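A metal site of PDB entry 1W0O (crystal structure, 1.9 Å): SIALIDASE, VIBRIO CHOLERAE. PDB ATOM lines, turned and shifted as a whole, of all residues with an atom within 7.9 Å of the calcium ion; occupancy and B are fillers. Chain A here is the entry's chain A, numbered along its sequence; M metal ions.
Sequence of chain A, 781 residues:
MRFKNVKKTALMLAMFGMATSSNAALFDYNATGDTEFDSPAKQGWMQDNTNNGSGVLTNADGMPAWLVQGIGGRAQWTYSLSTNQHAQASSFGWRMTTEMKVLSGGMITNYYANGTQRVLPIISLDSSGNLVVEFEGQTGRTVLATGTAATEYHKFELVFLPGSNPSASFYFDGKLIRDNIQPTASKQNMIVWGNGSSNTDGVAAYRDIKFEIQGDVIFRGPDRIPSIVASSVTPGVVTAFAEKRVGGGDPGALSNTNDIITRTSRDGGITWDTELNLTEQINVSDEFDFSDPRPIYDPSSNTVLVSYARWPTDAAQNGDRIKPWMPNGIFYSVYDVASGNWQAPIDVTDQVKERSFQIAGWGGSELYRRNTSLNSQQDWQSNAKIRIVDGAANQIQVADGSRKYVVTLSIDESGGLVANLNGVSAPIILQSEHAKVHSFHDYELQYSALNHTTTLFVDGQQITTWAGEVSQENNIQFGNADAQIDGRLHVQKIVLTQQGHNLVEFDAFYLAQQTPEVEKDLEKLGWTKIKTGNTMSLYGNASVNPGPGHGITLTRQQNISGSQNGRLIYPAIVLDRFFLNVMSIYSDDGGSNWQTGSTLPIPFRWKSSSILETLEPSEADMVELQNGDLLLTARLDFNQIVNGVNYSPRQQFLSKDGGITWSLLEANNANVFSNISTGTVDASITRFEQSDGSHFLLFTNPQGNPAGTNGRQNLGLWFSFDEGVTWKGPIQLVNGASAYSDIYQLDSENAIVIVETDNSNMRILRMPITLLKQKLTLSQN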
ATOM      1  N   ILE A 225     -32.905 -11.748   5.310  1.00  0.00           N
ATOM      2  CA  ILE A 225     -31.519 -11.788   5.796  1.00  0.00           C
ATOM      3  C   ILE A 225     -31.244 -10.931   7.027  1.00  0.00           C
ATOM      4  O   ILE A 225     -30.574  -9.905   6.939  1.00  0.00           O
ATOM      5  CB  ILE A 225     -30.554 -11.367   4.659  1.00  0.00           C
ATOM      6  CG1 ILE A 225     -31.061 -11.917   3.312  1.00  0.00           C
ATOM      7  CG2 ILE A 225     -29.146 -11.880   4.942  1.00  0.00           C
ATOM      8  CD1 ILE A 225     -31.354 -13.410   3.303  1.00  0.00           C
ATOM      9  N   PRO A 226     -31.741 -11.356   8.193  1.00  0.00           N
ATOM     10  CA  PRO A 226     -31.588 -10.658   9.473  1.00  0.00           C
ATOM     11  C   PRO A 226     -30.290 -10.873  10.239  1.00  0.00           C
ATOM     12  O   PRO A 226     -29.658 -11.926  10.153  1.00  0.00           O
ATOM     13  CB  PRO A 226     -32.793 -11.147  10.259  1.00  0.00           C
ATOM     14  CG  PRO A 226     -32.839 -12.604   9.852  1.00  0.00           C
ATOM     15  CD  PRO A 226     -32.630 -12.532   8.352  1.00  0.00           C
ATOM     16  N   SER A 227     -29.911  -9.848  11.003  1.00  0.00           N
ATOM     17  CA  SER A 227     -28.732  -9.889  11.856  1.00  0.00           C
ATOM     18  C   SER A 227     -29.022  -8.966  13.026  1.00  0.00           C
ATOM     19  O   SER A 227     -29.859  -8.060  12.922  1.00  0.00           O
ATOM     20  CB  SER A 227     -27.479  -9.425  11.099  1.00  0.00           C
ATOM     21  OG  SER A 227     -27.553  -8.068  10.719  1.00  0.00           O
ATOM     22  N   ARG A 294     -23.731  -7.188   8.118  1.00  0.00           N
ATOM     23  CA  ARG A 294     -22.905  -7.903   9.106  1.00  0.00           C
ATOM     24  C   ARG A 294     -22.466  -6.908  10.178  1.00  0.00           C
ATOM     25  O   ARG A 294     -21.424  -6.259  10.066  1.00  0.00           O
ATOM     26  CB  ARG A 294     -21.676  -8.510   8.408  1.00  0.00           C
ATOM     27  CG  ARG A 294     -20.663  -9.192   9.346  1.00  0.00           C
ATOM     28  CD  ARG A 294     -21.104 -10.586   9.782  1.00  0.00           C
ATOM     29  NE  ARG A 294     -20.998 -11.565   8.696  1.00  0.00           N
ATOM     30  CZ  ARG A 294     -21.315 -12.849   8.810  1.00  0.00           C
ATOM     31  NH1 ARG A 294     -21.179 -13.667   7.762  1.00  0.00           N
ATOM     32  NH2 ARG A 294     -21.768 -13.336   9.962  1.00  0.00           N
ATOM     33  N   GLY A 547     -21.542 -11.532   4.182  1.00  0.00           N
ATOM     34  CA  GLY A 547     -22.277 -12.724   4.594  1.00  0.00           C
ATOM     35  C   GLY A 547     -23.312 -12.367   5.643  1.00  0.00           C
ATOM     36  O   GLY A 547     -23.206 -11.295   6.264  1.00  0.00           O
ATOM     37  N   PRO A 548     -24.308 -13.230   5.898  1.00  0.00           N
ATOM     38  CA  PRO A 548     -25.376 -13.011   6.875  1.00  0.00           C
ATOM     39  C   PRO A 548     -25.117 -13.390   8.339  1.00  0.00           C
ATOM     40  O   PRO A 548     -24.770 -14.525   8.652  1.00  0.00           O
ATOM     41  CB  PRO A 548     -26.534 -13.815   6.297  1.00  0.00           C
ATOM     42  CG  PRO A 548     -25.820 -15.030   5.798  1.00  0.00           C
ATOM     43  CD  PRO A 548     -24.582 -14.447   5.106  1.00  0.00           C
ATOM     44  N   GLY A 549     -25.336 -12.419   9.226  1.00  0.00           N
ATOM     45  CA  GLY A 549     -25.146 -12.629  10.655  1.00  0.00           C
ATOM     46  C   GLY A 549     -24.390 -11.456  11.236  1.00  0.00           C
ATOM     47  O   GLY A 549     -24.367 -10.381  10.646  1.00  0.00           O
ATOM     48  N   HIS A 550     -23.769 -11.643  12.388  1.00  0.00           N
ATOM     49  CA  HIS A 550     -22.994 -10.567  13.012  1.00  0.00           C
ATOM     50  C   HIS A 550     -21.526 -10.946  13.080  1.00  0.00           C
ATOM     51  O   HIS A 550     -21.166 -12.103  12.907  1.00  0.00           O
ATOM     52  CB  HIS A 550     -23.544 -10.242  14.414  1.00  0.00           C
ATOM     53  CG  HIS A 550     -23.544 -11.417  15.348  1.00  0.00           C
ATOM     54  ND1 HIS A 550     -22.405 -11.871  15.973  1.00  0.00           N
ATOM     55  CD2 HIS A 550     -24.550 -12.231  15.745  1.00  0.00           C
ATOM     56  CE1 HIS A 550     -22.711 -12.909  16.727  1.00  0.00           C
ATOM     57  NE2 HIS A 550     -24.005 -13.157  16.608  1.00  0.00           N
ATOM     58  N   PRO A 571     -16.579 -13.428   9.052  1.00  0.00           N
ATOM     59  CA  PRO A 571     -16.261 -14.389   7.993  1.00  0.00           C
ATOM     60  C   PRO A 571     -17.001 -14.018   6.712  1.00  0.00           C
ATOM     61  O   PRO A 571     -18.206 -14.251   6.584  1.00  0.00           O
ATOM     62  CB  PRO A 571     -16.750 -15.702   8.581  1.00  0.00           C
ATOM     63  CG  PRO A 571     -17.987 -15.278   9.327  1.00  0.00           C
ATOM     64  CD  PRO A 571     -17.584 -13.967   9.976  1.00  0.00           C
ATOM     65  N   GLU A 619     -22.257 -18.907   3.584  1.00  0.00           N
ATOM     66  CA  GLU A 619     -22.760 -18.187   4.751  1.00  0.00           C
ATOM     67  C   GLU A 619     -22.204 -18.779   6.048  1.00  0.00           C
ATOM     68  O   GLU A 619     -22.531 -19.903   6.425  1.00  0.00           O
ATOM     69  CB  GLU A 619     -24.288 -18.220   4.732  1.00  0.00           C
ATOM     70  CG  GLU A 619     -24.839 -17.803   3.361  1.00  0.00           C
ATOM     71  CD  GLU A 619     -26.354 -17.839   3.273  1.00  0.00           C
ATOM     72  OE1 GLU A 619     -26.956 -18.747   3.869  1.00  0.00           O
ATOM     73  OE2 GLU A 619     -26.928 -16.981   2.575  1.00  0.00           O
ATOM     74  N   ALA A 620     -21.360 -17.993   6.720  1.00  0.00           N
ATOM     75  CA  ALA A 620     -20.693 -18.436   7.935  1.00  0.00           C
ATOM     76  C   ALA A 620     -20.837 -17.509   9.136  1.00  0.00           C
ATOM     77  O   ALA A 620     -21.196 -16.338   9.004  1.00  0.00           O
ATOM     78  CB  ALA A 620     -19.216 -18.654   7.642  1.00  0.00           C
ATOM     79  N   ASP A 621     -20.556 -18.044  10.319  1.00  0.00           N
ATOM     80  CA  ASP A 621     -20.639 -17.282  11.556  1.00  0.00           C
ATOM     81  C   ASP A 621     -19.515 -17.768  12.463  1.00  0.00           C
ATOM     82  O   ASP A 621     -19.174 -18.956  12.455  1.00  0.00           O
ATOM     83  CB  ASP A 621     -22.000 -17.507  12.216  1.00  0.00           C
ATOM     84  CG  ASP A 621     -23.145 -17.118  11.309  1.00  0.00           C
ATOM     85  OD1 ASP A 621     -23.501 -17.914  10.412  1.00  0.00           O
ATOM     86  OD2 ASP A 621     -23.699 -16.013  11.486  1.00  0.00           O
ATOM     87  N   MET A 622     -18.927 -16.867  13.242  1.00  0.00           N
ATOM     88  CA  MET A 622     -17.841 -17.273  14.129  1.00  0.00           C
ATOM     89  C   MET A 622     -17.994 -16.773  15.554  1.00  0.00           C
ATOM     90  O   MET A 622     -18.691 -15.792  15.808  1.00  0.00           O
ATOM     91  CB  MET A 622     -16.488 -16.804  13.569  1.00  0.00           C
ATOM     92  CG  MET A 622     -16.265 -15.290  13.577  1.00  0.00           C
ATOM     93  SD  MET A 622     -14.535 -14.819  13.288  1.00  0.00           S
ATOM     94  CE  MET A 622     -14.462 -14.871  11.495  1.00  0.00           C
ATOM     95  N   THR A 633     -18.527 -21.700  11.877  1.00  0.00           N
ATOM     96  CA  THR A 633     -19.471 -22.692  11.361  1.00  0.00           C
ATOM     97  C   THR A 633     -19.939 -22.161  10.024  1.00  0.00           C
ATOM     98  O   THR A 633     -20.391 -21.014   9.918  1.00  0.00           O
ATOM     99  CB  THR A 633     -20.668 -22.904  12.303  1.00  0.00           C
ATOM    100  OG1 THR A 633     -21.522 -23.918  11.770  1.00  0.00           O
ATOM    101  CG2 THR A 633     -21.464 -21.598  12.488  1.00  0.00           C
ATOM    102  N   ARG A 650     -23.241 -28.420   6.488  1.00  0.00           N
ATOM    103  CA  ARG A 650     -22.577 -27.481   7.398  1.00  0.00           C
ATOM    104  C   ARG A 650     -21.261 -28.065   7.914  1.00  0.00           C
ATOM    105  O   ARG A 650     -21.168 -29.265   8.189  1.00  0.00           O
ATOM    106  CB  ARG A 650     -23.503 -27.145   8.571  1.00  0.00           C
ATOM    107  CG  ARG A 650     -22.900 -26.226   9.632  1.00  0.00           C
ATOM    108  CD  ARG A 650     -24.003 -25.574  10.461  1.00  0.00           C
ATOM    109  NE  ARG A 650     -24.851 -24.730   9.610  1.00  0.00           N
ATOM    110  CZ  ARG A 650     -24.542 -23.496   9.234  1.00  0.00           C
ATOM    111  NH1 ARG A 650     -23.405 -22.922   9.621  1.00  0.00           N
ATOM    112  NH2 ARG A 650     -25.364 -22.822   8.443  1.00  0.00           N
ATOM    113  N   VAL A 681     -28.875 -23.758   4.808  1.00  0.00           N
ATOM    114  CA  VAL A 681     -29.496 -22.511   5.249  1.00  0.00           C
ATOM    115  C   VAL A 681     -28.540 -21.800   6.202  1.00  0.00           C
ATOM    116  O   VAL A 681     -27.650 -22.427   6.776  1.00  0.00           O
ATOM    117  CB  VAL A 681     -30.834 -22.812   5.976  1.00  0.00           C
ATOM    118  CG1 VAL A 681     -30.563 -23.658   7.215  1.00  0.00           C
ATOM    119  CG2 VAL A 681     -31.540 -21.515   6.347  1.00  0.00           C
ATOM    120  N   ASP A 682     -28.706 -20.487   6.360  1.00  0.00           N
ATOM    121  CA  ASP A 682     -27.830 -19.741   7.260  1.00  0.00           C
ATOM    122  C   ASP A 682     -28.175 -20.072   8.705  1.00  0.00           C
ATOM    123  O   ASP A 682     -29.335 -20.338   9.044  1.00  0.00           O
ATOM    124  CB  ASP A 682     -27.976 -18.226   7.047  1.00  0.00           C
ATOM    125  CG  ASP A 682     -27.030 -17.416   7.926  1.00  0.00           C
ATOM    126  OD1 ASP A 682     -25.830 -17.748   7.969  1.00  0.00           O
ATOM    127  OD2 ASP A 682     -27.493 -16.444   8.568  1.00  0.00           O
ATOM    128  N   ALA A 683     -27.158 -20.068   9.552  1.00  0.00           N
ATOM    129  CA  ALA A 683     -27.331 -20.359  10.971  1.00  0.00           C
ATOM    130  C   ALA A 683     -26.717 -19.192  11.743  1.00  0.00           C
ATOM    131  O   ALA A 683     -26.327 -18.191  11.158  1.00  0.00           O
ATOM    132  CB  ALA A 683     -26.631 -21.661  11.340  1.00  0.00           C
ATOM    133  N   SER A 684     -26.647 -19.345  13.065  1.00  0.00           N
ATOM    134  CA  SER A 684     -26.061 -18.323  13.912  1.00  0.00           C
ATOM    135  C   SER A 684     -25.384 -19.000  15.092  1.00  0.00           C
ATOM    136  O   SER A 684     -25.837 -20.039  15.550  1.00  0.00           O
ATOM    137  CB  SER A 684     -27.123 -17.345  14.410  1.00  0.00           C
ATOM    138  OG  SER A 684     -26.519 -16.341  15.204  1.00  0.00           O
ATOM    139  N   ILE A 685     -24.299 -18.395  15.568  1.00  0.00           N
ATOM    140  CA  ILE A 685     -23.582 -18.932  16.706  1.00  0.00           C
ATOM    141  C   ILE A 685     -23.085 -17.734  17.507  1.00  0.00           C
ATOM    142  O   ILE A 685     -22.741 -16.695  16.935  1.00  0.00           O
ATOM    143  CB  ILE A 685     -22.378 -19.799  16.251  1.00  0.00           C
ATOM    144  CG1 ILE A 685     -21.817 -20.575  17.446  1.00  0.00           C
ATOM    145  CG2 ILE A 685     -21.287 -18.925  15.625  1.00  0.00           C
ATOM    146  CD1 ILE A 685     -20.767 -21.622  17.060  1.00  0.00           C
ATOM    147  N   THR A 700     -28.327 -21.434  16.536  1.00  0.00           N
ATOM    148  CA  THR A 700     -29.704 -21.520  16.062  1.00  0.00           C
ATOM    149  C   THR A 700     -29.747 -21.926  14.594  1.00  0.00           C
ATOM    150  O   THR A 700     -28.896 -21.523  13.797  1.00  0.00           O
ATOM    151  CB  THR A 700     -30.479 -20.181  16.258  1.00  0.00           C
ATOM    152  OG1 THR A 700     -29.796 -19.112  15.570  1.00  0.00           O
ATOM    153  CG2 THR A 700     -30.578 -19.842  17.742  1.00  0.00           C
ATOM    154  N   TYR A 740     -33.583 -18.167   7.951  1.00  0.00           N
ATOM    155  CA  TYR A 740     -32.402 -17.487   8.464  1.00  0.00           C
ATOM    156  C   TYR A 740     -32.671 -16.901   9.858  1.00  0.00           C
ATOM    157  O   TYR A 740     -33.775 -16.440  10.138  1.00  0.00           O
ATOM    158  CB  TYR A 740     -31.984 -16.352   7.518  1.00  0.00           C
ATOM    159  CG  TYR A 740     -31.275 -16.798   6.253  1.00  0.00           C
ATOM    160  CD1 TYR A 740     -31.636 -17.976   5.593  1.00  0.00           C
ATOM    161  CD2 TYR A 740     -30.282 -16.004   5.679  1.00  0.00           C
ATOM    162  CE1 TYR A 740     -31.025 -18.347   4.398  1.00  0.00           C
ATOM    163  CE2 TYR A 740     -29.667 -16.367   4.489  1.00  0.00           C
ATOM    164  CZ  TYR A 740     -30.043 -17.539   3.853  1.00  0.00           C
ATOM    165  OH  TYR A 740     -29.432 -17.890   2.669  1.00  0.00           O
ATOM    166  N   SER A 741     -31.655 -16.923  10.724  1.00  0.00           N
ATOM    167  CA  SER A 741     -31.784 -16.407  12.081  1.00  0.00           C
ATOM    168  C   SER A 741     -30.455 -15.873  12.600  1.00  0.00           C
ATOM    169  O   SER A 741     -29.416 -16.134  12.013  1.00  0.00           O
ATOM    170  CB  SER A 741     -32.252 -17.522  13.006  1.00  0.00           C
ATOM    171  OG  SER A 741     -31.216 -18.484  13.176  1.00  0.00           O
ATOM    172  N   ASP A 742     -30.511 -15.133  13.701  1.00  0.00           N
ATOM    173  CA  ASP A 742     -29.291 -14.609  14.321  1.00  0.00           C
ATOM    174  C   ASP A 742     -29.584 -14.442  15.800  1.00  0.00           C
ATOM    175  O   ASP A 742     -30.617 -13.905  16.183  1.00  0.00           O
ATOM    176  CB  ASP A 742     -28.862 -13.273  13.699  1.00  0.00           C
ATOM    177  CG  ASP A 742     -27.370 -12.988  13.911  1.00  0.00           C
ATOM    178  OD1 ASP A 742     -26.551 -13.908  13.691  1.00  0.00           O
ATOM    179  OD2 ASP A 742     -27.016 -11.852  14.278  1.00  0.00           O
ATOM    180  N   ILE A 743     -28.680 -14.928  16.641  1.00  0.00           N
ATOM    181  CA  ILE A 743     -28.855 -14.828  18.082  1.00  0.00           C
ATOM    182  C   ILE A 743     -27.714 -14.022  18.693  1.00  0.00           C
ATOM    183  O   ILE A 743     -26.580 -14.085  18.212  1.00  0.00           O
ATOM    184  CB  ILE A 743     -28.914 -16.254  18.712  1.00  0.00           C
ATOM    185  CG1 ILE A 743     -29.228 -16.164  20.202  1.00  0.00           C
ATOM    186  CG2 ILE A 743     -27.589 -16.986  18.485  1.00  0.00           C
ATOM    187  CD1 ILE A 743     -29.594 -17.510  20.818  1.00  0.00           C
HETATM  188 CA    CA M   1     -25.457 -16.427   9.884  1.00  0.00          CA
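The calcium ion is bound by the backbone carbonyl oxygen (O) of Ala 683, the side-chain carboxylate (OD1) of Asp 682, the backbone carbonyl oxygen (O) of Pro 548, the side-chain carboxylate (OD2) of Asp 621, the side-chain carboxylate (OD2) of Asp 682 and the side-chain carboxylate (OD1) of Asp 621.
The calcium ion has six donor atoms within binding distance.
The side-chain carboxylate (OD2) of Asp 621 sits close to the guanidinium group (NH2) of Arg 294.
O of Pro 548 sits close to NH2 of Arg 294.
The backbone NH (N) of Thr 633 is in hydrogen-bond range of the backbone carbonyl oxygen (O) of Asp 621 (2.9 Å).
CA of Gly 549 touches the calcium ion (3.9 Å).
Five residues have an atom within 4 Å of the calcium ion: Pro 548, Gly 549, Asp 621, Asp 682 and Ala 683.
Along chain A the residues within 4 Å of the calcium ion span positions 548 to 683.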
